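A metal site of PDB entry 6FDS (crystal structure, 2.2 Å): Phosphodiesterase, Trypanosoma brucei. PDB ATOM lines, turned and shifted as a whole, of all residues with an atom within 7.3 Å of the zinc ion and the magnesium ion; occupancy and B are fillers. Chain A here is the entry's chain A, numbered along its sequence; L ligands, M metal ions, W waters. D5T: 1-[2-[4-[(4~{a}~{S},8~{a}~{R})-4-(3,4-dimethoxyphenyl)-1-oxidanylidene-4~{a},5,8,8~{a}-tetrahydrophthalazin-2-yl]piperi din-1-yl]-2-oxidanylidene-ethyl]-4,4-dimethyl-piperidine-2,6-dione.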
ATOM      1  N   TYR A 110      25.879  -9.863  22.917  1.00  0.00           N
ATOM      2  CA  TYR A 110      27.170  -9.163  23.119  1.00  0.00           C
ATOM      3  C   TYR A 110      27.466  -8.903  24.575  1.00  0.00           C
ATOM      4  O   TYR A 110      28.488  -9.359  25.070  1.00  0.00           O
ATOM      5  CB  TYR A 110      27.222  -7.836  22.344  1.00  0.00           C
ATOM      6  CG  TYR A 110      28.542  -7.090  22.489  1.00  0.00           C
ATOM      7  CD1 TYR A 110      29.639  -7.416  21.685  1.00  0.00           C
ATOM      8  CD2 TYR A 110      28.704  -6.064  23.428  1.00  0.00           C
ATOM      9  CE1 TYR A 110      30.862  -6.741  21.807  1.00  0.00           C
ATOM     10  CE2 TYR A 110      29.923  -5.399  23.569  1.00  0.00           C
ATOM     11  CZ  TYR A 110      31.001  -5.735  22.734  1.00  0.00           C
ATOM     12  OH  TYR A 110      32.187  -5.108  22.853  1.00  0.00           O
ATOM     13  N   HIS A 111      26.558  -8.190  25.263  1.00  0.00           N
ATOM     14  CA  HIS A 111      26.785  -7.807  26.647  1.00  0.00           C
ATOM     15  C   HIS A 111      26.563  -8.926  27.657  1.00  0.00           C
ATOM     16  O   HIS A 111      25.839  -8.769  28.623  1.00  0.00           O
ATOM     17  CB  HIS A 111      25.963  -6.599  26.995  1.00  0.00           C
ATOM     18  CG  HIS A 111      26.433  -5.348  26.339  1.00  0.00           C
ATOM     19  ND1 HIS A 111      25.771  -4.775  25.293  1.00  0.00           N
ATOM     20  CD2 HIS A 111      27.517  -4.573  26.572  1.00  0.00           C
ATOM     21  CE1 HIS A 111      26.402  -3.670  24.924  1.00  0.00           C
ATOM     22  NE2 HIS A 111      27.475  -3.527  25.678  1.00  0.00           N
ATOM     23  N   HIS A 115      32.027 -10.831  27.173  1.00  0.00           N
ATOM     24  CA  HIS A 115      32.438  -9.431  27.002  1.00  0.00           C
ATOM     25  C   HIS A 115      33.242  -8.964  28.172  1.00  0.00           C
ATOM     26  O   HIS A 115      34.336  -8.419  27.973  1.00  0.00           O
ATOM     27  CB  HIS A 115      31.219  -8.508  26.804  1.00  0.00           C
ATOM     28  CG  HIS A 115      31.525  -7.059  26.967  1.00  0.00           C
ATOM     29  ND1 HIS A 115      32.370  -6.369  26.124  1.00  0.00           N
ATOM     30  CD2 HIS A 115      31.093  -6.167  27.892  1.00  0.00           C
ATOM     31  CE1 HIS A 115      32.421  -5.109  26.511  1.00  0.00           C
ATOM     32  NE2 HIS A 115      31.671  -4.959  27.588  1.00  0.00           N
ATOM     33  N   VAL A 116      32.782  -9.221  29.387  1.00  0.00           N
ATOM     34  CA  VAL A 116      33.499  -8.686  30.580  1.00  0.00           C
ATOM     35  C   VAL A 116      34.781  -9.423  30.866  1.00  0.00           C
ATOM     36  O   VAL A 116      35.725  -8.832  31.317  1.00  0.00           O
ATOM     37  CB  VAL A 116      32.599  -8.519  31.849  1.00  0.00           C
ATOM     38  CG1 VAL A 116      31.381  -7.676  31.531  1.00  0.00           C
ATOM     39  CG2 VAL A 116      32.166  -9.819  32.457  1.00  0.00           C
ATOM     40  N   VAL A 119      37.144  -7.868  28.508  1.00  0.00           N
ATOM     41  CA  VAL A 119      37.594  -6.557  28.970  1.00  0.00           C
ATOM     42  C   VAL A 119      38.633  -6.742  30.040  1.00  0.00           C
ATOM     43  O   VAL A 119      39.660  -6.040  30.025  1.00  0.00           O
ATOM     44  CB  VAL A 119      36.451  -5.649  29.391  1.00  0.00           C
ATOM     45  CG1 VAL A 119      36.971  -4.357  30.048  1.00  0.00           C
ATOM     46  CG2 VAL A 119      35.559  -5.325  28.177  1.00  0.00           C
ATOM     47  N   ALA A 148      36.487  -4.552  35.638  1.00  0.00           N
ATOM     48  CA  ALA A 148      36.150  -5.147  34.367  1.00  0.00           C
ATOM     49  C   ALA A 148      34.981  -6.132  34.447  1.00  0.00           C
ATOM     50  O   ALA A 148      34.066  -6.146  33.589  1.00  0.00           O
ATOM     51  CB  ALA A 148      37.369  -5.879  33.801  1.00  0.00           C
ATOM     52  N   HIS A 151      31.454  -4.419  35.246  1.00  0.00           N
ATOM     53  CA  HIS A 151      31.130  -3.088  34.643  1.00  0.00           C
ATOM     54  C   HIS A 151      29.853  -3.025  33.834  1.00  0.00           C
ATOM     55  O   HIS A 151      29.424  -1.917  33.433  1.00  0.00           O
ATOM     56  CB  HIS A 151      32.331  -2.567  33.811  1.00  0.00           C
ATOM     57  CG  HIS A 151      32.368  -3.067  32.399  1.00  0.00           C
ATOM     58  ND1 HIS A 151      33.055  -4.201  32.017  1.00  0.00           N
ATOM     59  CD2 HIS A 151      31.803  -2.574  31.268  1.00  0.00           C
ATOM     60  CE1 HIS A 151      32.904  -4.392  30.712  1.00  0.00           C
ATOM     61  NE2 HIS A 151      32.127  -3.432  30.232  1.00  0.00           N
ATOM     62  N   ASP A 152      29.280  -4.217  33.534  1.00  0.00           N
ATOM     63  CA  ASP A 152      28.041  -4.349  32.770  1.00  0.00           C
ATOM     64  C   ASP A 152      27.028  -5.320  33.438  1.00  0.00           C
ATOM     65  O   ASP A 152      26.190  -5.914  32.750  1.00  0.00           O
ATOM     66  CB  ASP A 152      28.368  -4.879  31.349  1.00  0.00           C
ATOM     67  CG  ASP A 152      28.703  -3.764  30.342  1.00  0.00           C
ATOM     68  OD1 ASP A 152      28.238  -2.554  30.439  1.00  0.00           O
ATOM     69  OD2 ASP A 152      29.456  -4.156  29.418  1.00  0.00           O
ATOM     70  N   LEU A 153      27.082  -5.488  34.757  1.00  0.00           N
ATOM     71  CA  LEU A 153      26.206  -6.497  35.413  1.00  0.00           C
ATOM     72  C   LEU A 153      24.734  -6.303  35.073  1.00  0.00           C
ATOM     73  O   LEU A 153      24.266  -5.185  35.069  1.00  0.00           O
ATOM     74  CB  LEU A 153      26.357  -6.484  36.939  1.00  0.00           C
ATOM     75  CG  LEU A 153      27.653  -7.058  37.486  1.00  0.00           C
ATOM     76  CD1 LEU A 153      27.831  -6.584  38.913  1.00  0.00           C
ATOM     77  CD2 LEU A 153      27.826  -8.545  37.413  1.00  0.00           C
ATOM     78  N   HIS A 155      23.100  -6.532  32.243  1.00  0.00           N
ATOM     79  CA  HIS A 155      22.785  -5.896  30.953  1.00  0.00           C
ATOM     80  C   HIS A 155      21.738  -6.751  30.235  1.00  0.00           C
ATOM     81  O   HIS A 155      21.882  -7.973  30.175  1.00  0.00           O
ATOM     82  CB  HIS A 155      24.042  -5.757  30.093  1.00  0.00           C
ATOM     83  CG  HIS A 155      23.997  -4.634  29.118  1.00  0.00           C
ATOM     84  ND1 HIS A 155      23.120  -4.616  28.050  1.00  0.00           N
ATOM     85  CD2 HIS A 155      24.746  -3.513  29.007  1.00  0.00           C
ATOM     86  CE1 HIS A 155      23.290  -3.498  27.375  1.00  0.00           C
ATOM     87  NE2 HIS A 155      24.283  -2.816  27.924  1.00  0.00           N
ATOM     88  N   LEU A 183      21.952   2.542  32.814  1.00  0.00           N
ATOM     89  CA  LEU A 183      22.535   1.189  33.118  1.00  0.00           C
ATOM     90  C   LEU A 183      23.746   1.230  34.054  1.00  0.00           C
ATOM     91  O   LEU A 183      23.932   0.339  34.897  1.00  0.00           O
ATOM     92  CB  LEU A 183      22.943   0.477  31.842  1.00  0.00           C
ATOM     93  CG  LEU A 183      21.753   0.125  30.939  1.00  0.00           C
ATOM     94  CD1 LEU A 183      22.203  -0.035  29.484  1.00  0.00           C
ATOM     95  CD2 LEU A 183      21.119  -1.150  31.460  1.00  0.00           C
ATOM     96  N   GLU A 184      24.555   2.275  33.930  1.00  0.00           N
ATOM     97  CA  GLU A 184      25.813   2.320  34.663  1.00  0.00           C
ATOM     98  C   GLU A 184      25.549   2.456  36.165  1.00  0.00           C
ATOM     99  O   GLU A 184      26.104   1.710  36.985  1.00  0.00           O
ATOM    100  CB  GLU A 184      26.702   3.440  34.099  1.00  0.00           C
ATOM    101  CG  GLU A 184      27.146   3.179  32.663  1.00  0.00           C
ATOM    102  CD  GLU A 184      26.083   3.345  31.571  1.00  0.00           C
ATOM    103  OE1 GLU A 184      25.004   3.937  31.821  1.00  0.00           O
ATOM    104  OE2 GLU A 184      26.365   2.883  30.433  1.00  0.00           O
ATOM    105  N   HIS A 187      24.509  -1.020  37.116  1.00  0.00           N
ATOM    106  CA  HIS A 187      25.654  -1.945  37.277  1.00  0.00           C
ATOM    107  C   HIS A 187      26.395  -1.651  38.602  1.00  0.00           C
ATOM    108  O   HIS A 187      26.859  -2.543  39.299  1.00  0.00           O
ATOM    109  CB  HIS A 187      26.699  -1.882  36.118  1.00  0.00           C
ATOM    110  CG  HIS A 187      26.130  -1.875  34.718  1.00  0.00           C
ATOM    111  ND1 HIS A 187      25.253  -2.833  34.261  1.00  0.00           N
ATOM    112  CD2 HIS A 187      26.331  -1.027  33.677  1.00  0.00           C
ATOM    113  CE1 HIS A 187      24.918  -2.566  33.010  1.00  0.00           C
ATOM    114  NE2 HIS A 187      25.570  -1.482  32.627  1.00  0.00           N
ATOM    115  N   VAL A 222      33.132   2.508  36.338  1.00  0.00           N
ATOM    116  CA  VAL A 222      31.881   2.017  35.724  1.00  0.00           C
ATOM    117  C   VAL A 222      31.025   3.161  35.199  1.00  0.00           C
ATOM    118  O   VAL A 222      30.525   3.082  34.098  1.00  0.00           O
ATOM    119  CB  VAL A 222      31.055   1.224  36.715  1.00  0.00           C
ATOM    120  CG1 VAL A 222      29.717   0.847  36.100  1.00  0.00           C
ATOM    121  CG2 VAL A 222      31.798  -0.018  37.104  1.00  0.00           C
ATOM    122  N   THR A 225      32.097   4.518  31.831  1.00  0.00           N
ATOM    123  CA  THR A 225      31.773   3.713  30.655  1.00  0.00           C
ATOM    124  C   THR A 225      30.557   4.179  29.819  1.00  0.00           C
ATOM    125  O   THR A 225      30.364   3.675  28.691  1.00  0.00           O
ATOM    126  CB  THR A 225      31.654   2.215  30.950  1.00  0.00           C
ATOM    127  OG1 THR A 225      30.518   1.944  31.788  1.00  0.00           O
ATOM    128  CG2 THR A 225      32.900   1.715  31.609  1.00  0.00           C
ATOM    129  N   ASP A 226      29.764   5.108  30.314  1.00  0.00           N
ATOM    130  CA  ASP A 226      28.641   5.633  29.520  1.00  0.00           C
ATOM    131  C   ASP A 226      29.181   6.405  28.320  1.00  0.00           C
ATOM    132  O   ASP A 226      29.756   7.481  28.485  1.00  0.00           O
ATOM    133  CB  ASP A 226      27.718   6.507  30.419  1.00  0.00           C
ATOM    134  CG  ASP A 226      26.542   7.135  29.681  1.00  0.00           C
ATOM    135  OD1 ASP A 226      26.387   6.961  28.459  1.00  0.00           O
ATOM    136  OD2 ASP A 226      25.757   7.830  30.330  1.00  0.00           O
ATOM    137  N   MET A 227      28.983   5.888  27.111  1.00  0.00           N
ATOM    138  CA  MET A 227      29.513   6.541  25.888  1.00  0.00           C
ATOM    139  C   MET A 227      28.935   7.927  25.578  1.00  0.00           C
ATOM    140  O   MET A 227      29.494   8.658  24.725  1.00  0.00           O
ATOM    141  CB  MET A 227      29.347   5.631  24.681  1.00  0.00           C
ATOM    142  CG  MET A 227      30.291   4.432  24.650  1.00  0.00           C
ATOM    143  SD  MET A 227      32.076   4.865  24.743  1.00  0.00           S
ATOM    144  CE  MET A 227      32.250   5.299  23.010  1.00  0.00           C
ATOM    145  N   LEU A 260      39.664   1.432  31.535  1.00  0.00           N
ATOM    146  CA  LEU A 260      38.421   0.629  31.429  1.00  0.00           C
ATOM    147  C   LEU A 260      37.694   1.016  30.174  1.00  0.00           C
ATOM    148  O   LEU A 260      37.226   0.134  29.471  1.00  0.00           O
ATOM    149  CB  LEU A 260      37.501   0.812  32.651  1.00  0.00           C
ATOM    150  CG  LEU A 260      36.159   0.024  32.603  1.00  0.00           C
ATOM    151  CD1 LEU A 260      36.381  -1.475  32.616  1.00  0.00           C
ATOM    152  CD2 LEU A 260      35.270   0.366  33.761  1.00  0.00           C
ATOM    153  N   GLY A 263      39.487  -0.668  27.347  1.00  0.00           N
ATOM    154  CA  GLY A 263      39.110  -2.077  27.273  1.00  0.00           C
ATOM    155  C   GLY A 263      37.725  -2.278  26.640  1.00  0.00           C
ATOM    156  O   GLY A 263      37.506  -3.184  25.840  1.00  0.00           O
ATOM    157  N   ASP A 264      36.798  -1.401  26.996  1.00  0.00           N
ATOM    158  CA  ASP A 264      35.448  -1.491  26.555  1.00  0.00           C
ATOM    159  C   ASP A 264      35.299  -1.291  25.054  1.00  0.00           C
ATOM    160  O   ASP A 264      34.414  -1.845  24.464  1.00  0.00           O
ATOM    161  CB  ASP A 264      34.587  -0.421  27.293  1.00  0.00           C
ATOM    162  CG  ASP A 264      33.208  -0.918  27.654  1.00  0.00           C
ATOM    163  OD1 ASP A 264      32.973  -2.137  27.544  1.00  0.00           O
ATOM    164  OD2 ASP A 264      32.388  -0.054  28.022  1.00  0.00           O
ATOM    165  N   ILE A 265      36.173  -0.488  24.435  1.00  0.00           N
ATOM    166  CA  ILE A 265      36.130  -0.248  22.993  1.00  0.00           C
ATOM    167  C   ILE A 265      37.313  -0.891  22.298  1.00  0.00           C
ATOM    168  O   ILE A 265      37.694  -0.443  21.210  1.00  0.00           O
ATOM    169  CB  ILE A 265      36.002   1.232  22.609  1.00  0.00           C
ATOM    170  CG1 ILE A 265      37.181   2.074  23.056  1.00  0.00           C
ATOM    171  CG2 ILE A 265      34.690   1.833  23.155  1.00  0.00           C
ATOM    172  CD1 ILE A 265      37.055   3.521  22.647  1.00  0.00           C
HETATM  173  C1  D5T L   1      32.631  -4.361  17.451  1.00  0.00           C
HETATM  174  O1  D5T L   1      32.093  -3.058  17.179  1.00  0.00           O
HETATM  175  C2  D5T L   1      31.468  -2.377  18.191  1.00  0.00           C
HETATM  176  C3  D5T L   1      31.612  -2.641  19.544  1.00  0.00           C
HETATM  177  C4  D5T L   1      30.939  -1.884  20.486  1.00  0.00           C
HETATM  178  C5  D5T L   1      30.102  -0.841  20.090  1.00  0.00           C
HETATM  179  C6  D5T L   1      29.404   0.028  21.087  1.00  0.00           C
HETATM  180  N1  D5T L   1      28.803   1.093  20.671  1.00  0.00           N
HETATM  181  N2  D5T L   1      28.302   1.966  21.587  1.00  0.00           N
HETATM  182  C7  D5T L   1      28.032   3.320  21.044  1.00  0.00           C
HETATM  183  C8  D5T L   1      29.283   3.983  20.488  1.00  0.00           C
HETATM  184  C9  D5T L   1      28.949   5.352  19.911  1.00  0.00           C
HETATM  185  N3  D5T L   1      27.910   5.226  18.885  1.00  0.00           N
HETATM  186  C10 D5T L   1      28.015   5.546  17.565  1.00  0.00           C
HETATM  187  O2  D5T L   1      27.137   5.270  16.744  1.00  0.00           O
HETATM  188  C11 D5T L   1      29.282   6.231  17.051  1.00  0.00           C
HETATM  189  N4  D5T L   1      29.230   6.332  15.563  1.00  0.00           N
HETATM  190  C12 D5T L   1      28.849   7.564  15.013  1.00  0.00           C
HETATM  191  O3  D5T L   1      28.608   8.520  15.733  1.00  0.00           O
HETATM  192  C13 D5T L   1      28.770   7.681  13.518  1.00  0.00           C
HETATM  193  C14 D5T L   1      28.615   6.352  12.736  1.00  0.00           C
HETATM  194  C15 D5T L   1      28.901   6.580  11.244  1.00  0.00           C
HETATM  195  C16 D5T L   1      27.199   5.792  12.880  1.00  0.00           C
HETATM  196  C17 D5T L   1      29.621   5.373  13.322  1.00  0.00           C
HETATM  197  C18 D5T L   1      29.506   5.191  14.810  1.00  0.00           C
HETATM  198  O4  D5T L   1      29.601   4.093  15.321  1.00  0.00           O
HETATM  199  C19 D5T L   1      26.655   4.648  19.411  1.00  0.00           C
HETATM  200  C20 D5T L   1      26.888   3.273  20.023  1.00  0.00           C
HETATM  201  C21 D5T L   1      28.001   1.705  22.904  1.00  0.00           C
HETATM  202  O5  D5T L   1      27.616   2.575  23.662  1.00  0.00           O
HETATM  203  C22 D5T L   1      28.250   0.262  23.286  1.00  0.00           C
HETATM  204  C23 D5T L   1      28.331  -0.004  24.793  1.00  0.00           C
HETATM  205  C24 D5T L   1      29.603   0.492  25.366  1.00  0.00           C
HETATM  206  C25 D5T L   1      30.670   0.756  24.642  1.00  0.00           C
HETATM  207  C26 D5T L   1      30.732   0.532  23.171  1.00  0.00           C
HETATM  208  C27 D5T L   1      29.529  -0.239  22.582  1.00  0.00           C
HETATM  209  C28 D5T L   1      29.957  -0.576  18.727  1.00  0.00           C
HETATM  210  C29 D5T L   1      30.629  -1.332  17.775  1.00  0.00           C
HETATM  211  O6  D5T L   1      30.545  -1.167  16.407  1.00  0.00           O
HETATM  212  C30 D5T L   1      29.690  -0.148  15.868  1.00  0.00           C
HETATM  213 ZN    ZN M   1      31.048  -3.119  28.342  1.00  0.00          ZN
HETATM  214 MG    MG M   2      28.305  -0.846  29.627  1.00  0.00          MG
HETATM  215  O   HOH W   1      30.175  -1.372  28.837  1.00  0.00           O
HETATM  216  O   HOH W   2      26.496  -0.490  30.041  1.00  0.00           O
HETATM  217  O   HOH W   3      28.373   0.933  29.186  1.00  0.00           O
HETATM  218  O   HOH W   4      29.928  -2.432  26.457  1.00  0.00           O
HETATM  219  O   HOH W   5      27.576  -1.208  27.840  1.00  0.00           O
HETATM  220  O   HOH W   6      28.919  -0.249  31.407  1.00  0.00           O
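The backbone carbonyl oxygen (O) of Ala 148 sits at hydrogen-bond distance from a ring nitrogen (ND1) of His 151, at 2.7 Å.
The nearest printed residue that does not touch the zinc ion is His 111 (4.2 Å).
The nearest printed residue that does not touch the magnesium ion is His 187 (4.1 Å).
The zinc ion is bound by water W1. NE2 of His 115 is bound to the zinc ion (2.1 Å). OD2 of Asp 152 binds the zinc ion, 2.2 Å away. NE2 of His 151 binds the zinc ion, at 2.2 Å. Water W4 binds the zinc ion, at 2.3 Å. The zinc ion is bound by OD1 of Asp 264. The zinc ion has six donor atoms within binding distance.
The magnesium ion is bound by water W3, water W2, the side-chain carboxylate of Asp 152, water W5, water W6 and water W1.
Water W6 lies within hydrogen-bond range of O of His 151 (2.7 Å) and OG1 of Thr 225 (2.7 Å). Water W2 bridges a ring nitrogen (NE2) of His 187 (2.9 Å) and the side-chain carboxylate of Glu 184 (3.4 Å). Water W3 bridges the side-chain carboxylate of Glu 184 (3.1 Å) and the backbone carbonyl oxygen of Thr 225 (3.4 Å).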
